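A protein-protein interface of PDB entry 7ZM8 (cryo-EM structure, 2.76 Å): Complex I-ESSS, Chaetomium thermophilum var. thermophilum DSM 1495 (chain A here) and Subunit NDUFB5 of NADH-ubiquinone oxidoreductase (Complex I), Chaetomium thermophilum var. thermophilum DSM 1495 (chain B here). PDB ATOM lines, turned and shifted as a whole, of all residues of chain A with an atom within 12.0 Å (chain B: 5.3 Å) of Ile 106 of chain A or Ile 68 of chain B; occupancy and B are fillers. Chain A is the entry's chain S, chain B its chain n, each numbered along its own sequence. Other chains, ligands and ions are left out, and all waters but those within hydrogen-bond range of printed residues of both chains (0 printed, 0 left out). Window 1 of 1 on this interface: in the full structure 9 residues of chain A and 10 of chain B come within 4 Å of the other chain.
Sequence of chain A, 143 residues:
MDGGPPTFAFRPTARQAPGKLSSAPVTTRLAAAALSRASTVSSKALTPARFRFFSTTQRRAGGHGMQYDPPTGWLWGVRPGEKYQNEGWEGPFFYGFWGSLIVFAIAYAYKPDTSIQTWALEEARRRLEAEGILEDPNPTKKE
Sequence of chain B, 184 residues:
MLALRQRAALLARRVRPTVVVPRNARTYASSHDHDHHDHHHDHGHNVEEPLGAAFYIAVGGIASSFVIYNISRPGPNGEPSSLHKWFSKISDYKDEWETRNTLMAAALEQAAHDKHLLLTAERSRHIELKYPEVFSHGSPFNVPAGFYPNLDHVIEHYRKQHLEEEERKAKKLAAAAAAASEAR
Hydrophobic or aromatic side chains of chain A that line the printed part of chain B: Ile 106, Ala 109 and Tyr 110. Of the 10 printed residues of chain B, 3 touch a printed residue of chain A. Hydrophobic or aromatic side chains of chain B within 4 Å of the printed part of chain A: Ile 68 and Ile 71. Along chain B the printed residues that touch a printed residue of chain A span positions 68 to 72. Among the printed residues, 4 pairs touch across the chains.
CD1 of Ile 106 of chain A touches CD1 of Ile 68 of chain B, 3.9 Å away. Ala 109 of chain A touches Ser 72 of chain B (CB to OG, 3.4 Å). Ile 71 of chain B touches Tyr 110 of chain A (CG2 to OH, 3.8 Å). Ser 72 of chain B touches Tyr 110 of chain A.
Ser 100 of chain A touches none of the printed residues of chain B. Ile 106 of chain A touches just one residue of chain B: Ile 68 (3.9 Å). Of the printed residues of chain B, Ala 109 of chain A touches Ser 72. Printed residues of chain B within 4 Å of Tyr 110 of chain A: Ile 71 and Ser 72. No residue of chain A comes within 4 Å of Ser 64 of chain B. Ser 65 of chain B touches none of the printed residues of chain A. Val 67 of chain B touches none of the printed residues of chain A. Printed residues of chain A within 4 Å of Ile 68 of chain B: Ile 106. No residue of chain A comes within 4 Å of Asn 70 of chain B. Ile 71 of chain B touches just one residue of chain A: Tyr 110 (3.8 Å). The nearest printed residue of chain B that does not touch Ile 106 of chain A is Ser 72 of chain B (5.9 Å). The nearest residue of chain A that does not touch Ile 68 of chain B is Tyr 110 of chain A (4.8 Å).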
ATOM      1  N   TYR A  95      20.051   1.392 -13.106  1.00  0.00           N
ATOM      2  CA  TYR A  95      19.808   1.582 -14.529  1.00  0.00           C
ATOM      3  C   TYR A  95      20.342   0.434 -15.370  1.00  0.00           C
ATOM      4  O   TYR A  95      19.675  -0.005 -16.310  1.00  0.00           O
ATOM      5  CB  TYR A  95      20.441   2.893 -14.991  1.00  0.00           C
ATOM      6  CG  TYR A  95      19.798   4.110 -14.396  1.00  0.00           C
ATOM      7  CD1 TYR A  95      18.425   4.187 -14.249  1.00  0.00           C
ATOM      8  CD2 TYR A  95      20.562   5.182 -13.974  1.00  0.00           C
ATOM      9  CE1 TYR A  95      17.829   5.301 -13.702  1.00  0.00           C
ATOM     10  CE2 TYR A  95      19.978   6.302 -13.427  1.00  0.00           C
ATOM     11  CZ  TYR A  95      18.609   6.355 -13.294  1.00  0.00           C
ATOM     12  OH  TYR A  95      18.018   7.470 -12.747  1.00  0.00           O
ATOM     13  N   PHE A  97      21.999  -2.790 -14.163  1.00  0.00           N
ATOM     14  CA  PHE A  97      21.745  -4.145 -13.689  1.00  0.00           C
ATOM     15  C   PHE A  97      20.256  -4.456 -13.716  1.00  0.00           C
ATOM     16  O   PHE A  97      19.823  -5.401 -14.378  1.00  0.00           O
ATOM     17  CB  PHE A  97      22.319  -4.338 -12.288  1.00  0.00           C
ATOM     18  CG  PHE A  97      22.174  -5.736 -11.769  1.00  0.00           C
ATOM     19  CD1 PHE A  97      23.088  -6.712 -12.114  1.00  0.00           C
ATOM     20  CD2 PHE A  97      21.120  -6.075 -10.944  1.00  0.00           C
ATOM     21  CE1 PHE A  97      22.954  -7.995 -11.642  1.00  0.00           C
ATOM     22  CE2 PHE A  97      20.981  -7.355 -10.476  1.00  0.00           C
ATOM     23  CZ  PHE A  97      21.895  -8.317 -10.826  1.00  0.00           C
ATOM     24  N   TRP A  98      19.450  -3.660 -13.019  1.00  0.00           N
ATOM     25  CA  TRP A  98      18.020  -3.944 -13.000  1.00  0.00           C
ATOM     26  C   TRP A  98      17.369  -3.597 -14.327  1.00  0.00           C
ATOM     27  O   TRP A  98      16.536  -4.359 -14.823  1.00  0.00           O
ATOM     28  CB  TRP A  98      17.346  -3.211 -11.848  1.00  0.00           C
ATOM     29  CG  TRP A  98      17.424  -3.998 -10.594  1.00  0.00           C
ATOM     30  CD1 TRP A  98      18.249  -3.775  -9.539  1.00  0.00           C
ATOM     31  CD2 TRP A  98      16.672  -5.171 -10.277  1.00  0.00           C
ATOM     32  NE1 TRP A  98      18.047  -4.726  -8.573  1.00  0.00           N
ATOM     33  CE2 TRP A  98      17.082  -5.594  -9.004  1.00  0.00           C
ATOM     34  CE3 TRP A  98      15.683  -5.899 -10.944  1.00  0.00           C
ATOM     35  CZ2 TRP A  98      16.539  -6.710  -8.383  1.00  0.00           C
ATOM     36  CZ3 TRP A  98      15.149  -7.004 -10.330  1.00  0.00           C
ATOM     37  CH2 TRP A  98      15.577  -7.401  -9.061  1.00  0.00           C
ATOM     38  N   GLY A  99      17.768  -2.481 -14.938  1.00  0.00           N
ATOM     39  CA  GLY A  99      17.206  -2.121 -16.229  1.00  0.00           C
ATOM     40  C   GLY A  99      17.389  -3.211 -17.267  1.00  0.00           C
ATOM     41  O   GLY A  99      16.497  -3.467 -18.076  1.00  0.00           O
ATOM     42  N   SER A 100      18.543  -3.876 -17.249  1.00  0.00           N
ATOM     43  CA  SER A 100      18.777  -4.972 -18.180  1.00  0.00           C
ATOM     44  C   SER A 100      17.815  -6.127 -17.940  1.00  0.00           C
ATOM     45  O   SER A 100      17.425  -6.810 -18.891  1.00  0.00           O
ATOM     46  CB  SER A 100      20.221  -5.453 -18.069  1.00  0.00           C
ATOM     47  OG  SER A 100      20.583  -6.256 -19.177  1.00  0.00           O
ATOM     48  N   LEU A 101      17.430  -6.366 -16.685  1.00  0.00           N
ATOM     49  CA  LEU A 101      16.534  -7.478 -16.374  1.00  0.00           C
ATOM     50  C   LEU A 101      15.096  -7.202 -16.798  1.00  0.00           C
ATOM     51  O   LEU A 101      14.410  -8.114 -17.265  1.00  0.00           O
ATOM     52  CB  LEU A 101      16.612  -7.815 -14.888  1.00  0.00           C
ATOM     53  CG  LEU A 101      17.683  -8.822 -14.453  1.00  0.00           C
ATOM     54  CD1 LEU A 101      19.092  -8.317 -14.628  1.00  0.00           C
ATOM     55  CD2 LEU A 101      17.452  -9.191 -13.002  1.00  0.00           C
ATOM     56  N   ILE A 102      14.602  -5.973 -16.623  1.00  0.00           N
ATOM     57  CA  ILE A 102      13.278  -5.658 -17.161  1.00  0.00           C
ATOM     58  C   ILE A 102      13.284  -5.724 -18.682  1.00  0.00           C
ATOM     59  O   ILE A 102      12.351  -6.254 -19.295  1.00  0.00           O
ATOM     60  CB  ILE A 102      12.752  -4.295 -16.665  1.00  0.00           C
ATOM     61  CG1 ILE A 102      12.537  -4.266 -15.147  1.00  0.00           C
ATOM     62  CG2 ILE A 102      11.468  -3.919 -17.385  1.00  0.00           C
ATOM     63  CD1 ILE A 102      13.702  -3.849 -14.327  1.00  0.00           C
ATOM     64  N   VAL A 103      14.321  -5.183 -19.316  1.00  0.00           N
ATOM     65  CA  VAL A 103      14.406  -5.253 -20.771  1.00  0.00           C
ATOM     66  C   VAL A 103      14.578  -6.698 -21.226  1.00  0.00           C
ATOM     67  O   VAL A 103      14.077  -7.091 -22.284  1.00  0.00           O
ATOM     68  CB  VAL A 103      15.540  -4.345 -21.278  1.00  0.00           C
ATOM     69  CG1 VAL A 103      15.712  -4.488 -22.779  1.00  0.00           C
ATOM     70  CG2 VAL A 103      15.233  -2.912 -20.930  1.00  0.00           C
ATOM     71  N   PHE A 104      15.287  -7.507 -20.440  1.00  0.00           N
ATOM     72  CA  PHE A 104      15.360  -8.933 -20.730  1.00  0.00           C
ATOM     73  C   PHE A 104      14.008  -9.602 -20.534  1.00  0.00           C
ATOM     74  O   PHE A 104      13.642 -10.507 -21.290  1.00  0.00           O
ATOM     75  CB  PHE A 104      16.421  -9.596 -19.854  1.00  0.00           C
ATOM     76  CG  PHE A 104      16.362 -11.092 -19.865  1.00  0.00           C
ATOM     77  CD1 PHE A 104      16.913 -11.810 -20.904  1.00  0.00           C
ATOM     78  CD2 PHE A 104      15.741 -11.781 -18.838  1.00  0.00           C
ATOM     79  CE1 PHE A 104      16.851 -13.174 -20.916  1.00  0.00           C
ATOM     80  CE2 PHE A 104      15.670 -13.147 -18.853  1.00  0.00           C
ATOM     81  CZ  PHE A 104      16.227 -13.842 -19.887  1.00  0.00           C
ATOM     82  N   ALA A 105      13.256  -9.180 -19.517  1.00  0.00           N
ATOM     83  CA  ALA A 105      11.951  -9.774 -19.254  1.00  0.00           C
ATOM     84  C   ALA A 105      10.955  -9.466 -20.366  1.00  0.00           C
ATOM     85  O   ALA A 105      10.211 -10.350 -20.800  1.00  0.00           O
ATOM     86  CB  ALA A 105      11.418  -9.289 -17.909  1.00  0.00           C
ATOM     87  N   ILE A 106      10.923  -8.222 -20.842  1.00  0.00           N
ATOM     88  CA  ILE A 106       9.992  -7.885 -21.912  1.00  0.00           C
ATOM     89  C   ILE A 106      10.397  -8.570 -23.210  1.00  0.00           C
ATOM     90  O   ILE A 106       9.543  -9.007 -23.990  1.00  0.00           O
ATOM     91  CB  ILE A 106       9.872  -6.358 -22.071  1.00  0.00           C
ATOM     92  CG1 ILE A 106       8.765  -6.017 -23.067  1.00  0.00           C
ATOM     93  CG2 ILE A 106      11.178  -5.741 -22.506  1.00  0.00           C
ATOM     94  CD1 ILE A 106       8.345  -4.568 -23.037  1.00  0.00           C
ATOM     95  N   ALA A 107      11.701  -8.682 -23.463  1.00  0.00           N
ATOM     96  CA  ALA A 107      12.158  -9.381 -24.656  1.00  0.00           C
ATOM     97  C   ALA A 107      11.827 -10.864 -24.586  1.00  0.00           C
ATOM     98  O   ALA A 107      11.441 -11.465 -25.592  1.00  0.00           O
ATOM     99  CB  ALA A 107      13.658  -9.175 -24.840  1.00  0.00           C
ATOM    100  N   TYR A 108      11.969 -11.468 -23.406  1.00  0.00           N
ATOM    101  CA  TYR A 108      11.737 -12.898 -23.260  1.00  0.00           C
ATOM    102  C   TYR A 108      10.320 -13.300 -23.637  1.00  0.00           C
ATOM    103  O   TYR A 108      10.096 -14.454 -24.012  1.00  0.00           O
ATOM    104  CB  TYR A 108      12.036 -13.337 -21.830  1.00  0.00           C
ATOM    105  CG  TYR A 108      12.150 -14.834 -21.704  1.00  0.00           C
ATOM    106  CD1 TYR A 108      13.269 -15.503 -22.172  1.00  0.00           C
ATOM    107  CD2 TYR A 108      11.122 -15.579 -21.152  1.00  0.00           C
ATOM    108  CE1 TYR A 108      13.364 -16.865 -22.077  1.00  0.00           C
ATOM    109  CE2 TYR A 108      11.210 -16.940 -21.057  1.00  0.00           C
ATOM    110  CZ  TYR A 108      12.335 -17.581 -21.520  1.00  0.00           C
ATOM    111  OH  TYR A 108      12.436 -18.947 -21.424  1.00  0.00           O
ATOM    112  N   ALA A 109       9.365 -12.373 -23.558  1.00  0.00           N
ATOM    113  CA  ALA A 109       7.996 -12.673 -23.955  1.00  0.00           C
ATOM    114  C   ALA A 109       7.892 -12.966 -25.447  1.00  0.00           C
ATOM    115  O   ALA A 109       7.105 -13.821 -25.864  1.00  0.00           O
ATOM    116  CB  ALA A 109       7.081 -11.515 -23.577  1.00  0.00           C
ATOM    117  N   TYR A 110       8.661 -12.262 -26.265  1.00  0.00           N
ATOM    118  CA  TYR A 110       8.618 -12.453 -27.705  1.00  0.00           C
ATOM    119  C   TYR A 110       9.660 -13.437 -28.203  1.00  0.00           C
ATOM    120  O   TYR A 110       9.745 -13.664 -29.413  1.00  0.00           O
ATOM    121  CB  TYR A 110       8.792 -11.118 -28.419  1.00  0.00           C
ATOM    122  CG  TYR A 110       7.815 -10.075 -27.961  1.00  0.00           C
ATOM    123  CD1 TYR A 110       8.114  -9.235 -26.901  1.00  0.00           C
ATOM    124  CD2 TYR A 110       6.589  -9.931 -28.585  1.00  0.00           C
ATOM    125  CE1 TYR A 110       7.220  -8.283 -26.481  1.00  0.00           C
ATOM    126  CE2 TYR A 110       5.691  -8.981 -28.174  1.00  0.00           C
ATOM    127  CZ  TYR A 110       6.010  -8.159 -27.123  1.00  0.00           C
ATOM    128  OH  TYR A 110       5.112  -7.207 -26.707  1.00  0.00           O
ATOM    129  N   LYS A 111      10.446 -14.017 -27.312  1.00  0.00           N
ATOM    130  CA  LYS A 111      11.341 -15.094 -27.699  1.00  0.00           C
ATOM    131  C   LYS A 111      10.520 -16.255 -28.248  1.00  0.00           C
ATOM    132  O   LYS A 111       9.566 -16.695 -27.592  1.00  0.00           O
ATOM    133  CB  LYS A 111      12.166 -15.552 -26.497  1.00  0.00           C
ATOM    134  CG  LYS A 111      13.327 -16.458 -26.836  1.00  0.00           C
ATOM    135  CD  LYS A 111      13.782 -17.232 -25.610  1.00  0.00           C
ATOM    136  CE  LYS A 111      15.155 -17.858 -25.806  1.00  0.00           C
ATOM    137  NZ  LYS A 111      15.219 -18.724 -27.009  1.00  0.00           N
ATOM    138  N   PRO A 112      10.824 -16.751 -29.443  1.00  0.00           N
ATOM    139  CA  PRO A 112      10.122 -17.936 -29.941  1.00  0.00           C
ATOM    140  C   PRO A 112      10.418 -19.143 -29.069  1.00  0.00           C
ATOM    141  O   PRO A 112      11.494 -19.262 -28.480  1.00  0.00           O
ATOM    142  CB  PRO A 112      10.679 -18.110 -31.357  1.00  0.00           C
ATOM    143  CG  PRO A 112      11.913 -17.294 -31.396  1.00  0.00           C
ATOM    144  CD  PRO A 112      11.722 -16.175 -30.451  1.00  0.00           C
ATOM    145  N   ALA B  63       0.966  -3.962 -12.354  1.00  0.00           N
ATOM    146  CA  ALA B  63       0.215  -3.405 -13.471  1.00  0.00           C
ATOM    147  C   ALA B  63       0.968  -3.572 -14.784  1.00  0.00           C
ATOM    148  O   ALA B  63       0.375  -3.943 -15.802  1.00  0.00           O
ATOM    149  CB  ALA B  63      -0.093  -1.931 -13.210  1.00  0.00           C
ATOM    150  N   SER B  64       2.275  -3.304 -14.780  1.00  0.00           N
ATOM    151  CA  SER B  64       3.056  -3.443 -16.004  1.00  0.00           C
ATOM    152  C   SER B  64       3.072  -4.886 -16.484  1.00  0.00           C
ATOM    153  O   SER B  64       2.942  -5.149 -17.685  1.00  0.00           O
ATOM    154  CB  SER B  64       4.481  -2.937 -15.783  1.00  0.00           C
ATOM    155  OG  SER B  64       4.520  -1.521 -15.760  1.00  0.00           O
ATOM    156  N   SER B  65       3.232  -5.834 -15.560  1.00  0.00           N
ATOM    157  CA  SER B  65       3.268  -7.241 -15.942  1.00  0.00           C
ATOM    158  C   SER B  65       1.963  -7.662 -16.599  1.00  0.00           C
ATOM    159  O   SER B  65       1.968  -8.380 -17.605  1.00  0.00           O
ATOM    160  CB  SER B  65       3.554  -8.103 -14.715  1.00  0.00           C
ATOM    161  OG  SER B  65       4.825  -7.801 -14.169  1.00  0.00           O
ATOM    162  N   PHE B  66       0.835  -7.224 -16.044  1.00  0.00           N
ATOM    163  CA  PHE B  66      -0.455  -7.526 -16.651  1.00  0.00           C
ATOM    164  C   PHE B  66      -0.571  -6.892 -18.032  1.00  0.00           C
ATOM    165  O   PHE B  66      -1.110  -7.503 -18.961  1.00  0.00           O
ATOM    166  CB  PHE B  66      -1.578  -7.046 -15.731  1.00  0.00           C
ATOM    167  CG  PHE B  66      -2.943  -7.103 -16.349  1.00  0.00           C
ATOM    168  CD1 PHE B  66      -3.511  -8.317 -16.692  1.00  0.00           C
ATOM    169  CD2 PHE B  66      -3.664  -5.943 -16.572  1.00  0.00           C
ATOM    170  CE1 PHE B  66      -4.771  -8.371 -17.254  1.00  0.00           C
ATOM    171  CE2 PHE B  66      -4.924  -5.991 -17.133  1.00  0.00           C
ATOM    172  CZ  PHE B  66      -5.478  -7.207 -17.476  1.00  0.00           C
ATOM    173  N   VAL B  67      -0.068  -5.669 -18.186  1.00  0.00           N
ATOM    174  CA  VAL B  67      -0.140  -4.987 -19.474  1.00  0.00           C
ATOM    175  C   VAL B  67       0.781  -5.654 -20.489  1.00  0.00           C
ATOM    176  O   VAL B  67       0.390  -5.909 -21.631  1.00  0.00           O
ATOM    177  CB  VAL B  67       0.194  -3.496 -19.303  1.00  0.00           C
ATOM    178  CG1 VAL B  67       0.404  -2.839 -20.656  1.00  0.00           C
ATOM    179  CG2 VAL B  67      -0.911  -2.797 -18.535  1.00  0.00           C
ATOM    180  N   ILE B  68       2.022  -5.938 -20.087  1.00  0.00           N
ATOM    181  CA  ILE B  68       3.001  -6.494 -21.019  1.00  0.00           C
ATOM    182  C   ILE B  68       2.586  -7.889 -21.465  1.00  0.00           C
ATOM    183  O   ILE B  68       2.693  -8.237 -22.646  1.00  0.00           O
ATOM    184  CB  ILE B  68       4.402  -6.496 -20.381  1.00  0.00           C
ATOM    185  CG1 ILE B  68       4.920  -5.066 -20.232  1.00  0.00           C
ATOM    186  CG2 ILE B  68       5.369  -7.316 -21.214  1.00  0.00           C
ATOM    187  CD1 ILE B  68       4.769  -4.226 -21.479  1.00  0.00           C
ATOM    188  N   TYR B  69       2.111  -8.711 -20.530  1.00  0.00           N
ATOM    189  CA  TYR B  69       1.682 -10.059 -20.882  1.00  0.00           C
ATOM    190  C   TYR B  69       0.503 -10.031 -21.845  1.00  0.00           C
ATOM    191  O   TYR B  69       0.427 -10.849 -22.768  1.00  0.00           O
ATOM    192  CB  TYR B  69       1.323 -10.842 -19.621  1.00  0.00           C
ATOM    193  CG  TYR B  69       1.132 -12.317 -19.861  1.00  0.00           C
ATOM    194  CD1 TYR B  69       2.219 -13.156 -20.034  1.00  0.00           C
ATOM    195  CD2 TYR B  69      -0.138 -12.867 -19.920  1.00  0.00           C
ATOM    196  CE1 TYR B  69       2.047 -14.505 -20.256  1.00  0.00           C
ATOM    197  CE2 TYR B  69      -0.320 -14.213 -20.140  1.00  0.00           C
ATOM    198  CZ  TYR B  69       0.775 -15.029 -20.308  1.00  0.00           C
ATOM    199  OH  TYR B  69       0.595 -16.374 -20.528  1.00  0.00           O
ATOM    200  N   ASN B  70      -0.433  -9.104 -21.639  1.00  0.00           N
ATOM    201  CA  ASN B  70      -1.590  -9.014 -22.523  1.00  0.00           C
ATOM    202  C   ASN B  70      -1.175  -8.659 -23.944  1.00  0.00           C
ATOM    203  O   ASN B  70      -1.728  -9.192 -24.912  1.00  0.00           O
ATOM    204  CB  ASN B  70      -2.579  -7.987 -21.980  1.00  0.00           C
ATOM    205  CG  ASN B  70      -3.433  -8.540 -20.863  1.00  0.00           C
ATOM    206  OD1 ASN B  70      -2.999  -9.412 -20.113  1.00  0.00           O
ATOM    207  ND2 ASN B  70      -4.656  -8.036 -20.745  1.00  0.00           N
ATOM    208  N   ILE B  71      -0.207  -7.754 -24.090  1.00  0.00           N
ATOM    209  CA  ILE B  71       0.206  -7.314 -25.417  1.00  0.00           C
ATOM    210  C   ILE B  71       0.932  -8.432 -26.159  1.00  0.00           C
ATOM    211  O   ILE B  71       0.696  -8.654 -27.354  1.00  0.00           O
ATOM    212  CB  ILE B  71       1.075  -6.049 -25.309  1.00  0.00           C
ATOM    213  CG1 ILE B  71       0.259  -4.892 -24.735  1.00  0.00           C
ATOM    214  CG2 ILE B  71       1.640  -5.672 -26.666  1.00  0.00           C
ATOM    215  CD1 ILE B  71      -1.015  -4.609 -25.498  1.00  0.00           C
ATOM    216  N   SER B  72       1.812  -9.153 -25.472  1.00  0.00           N
ATOM    217  CA  SER B  72       2.712 -10.104 -26.114  1.00  0.00           C
ATOM    218  C   SER B  72       2.076 -11.460 -26.391  1.00  0.00           C
ATOM    219  O   SER B  72       2.808 -12.423 -26.632  1.00  0.00           O
ATOM    220  CB  SER B  72       3.965 -10.297 -25.259  1.00  0.00           C
ATOM    221  OG  SER B  72       3.731 -11.232 -24.223  1.00  0.00           O
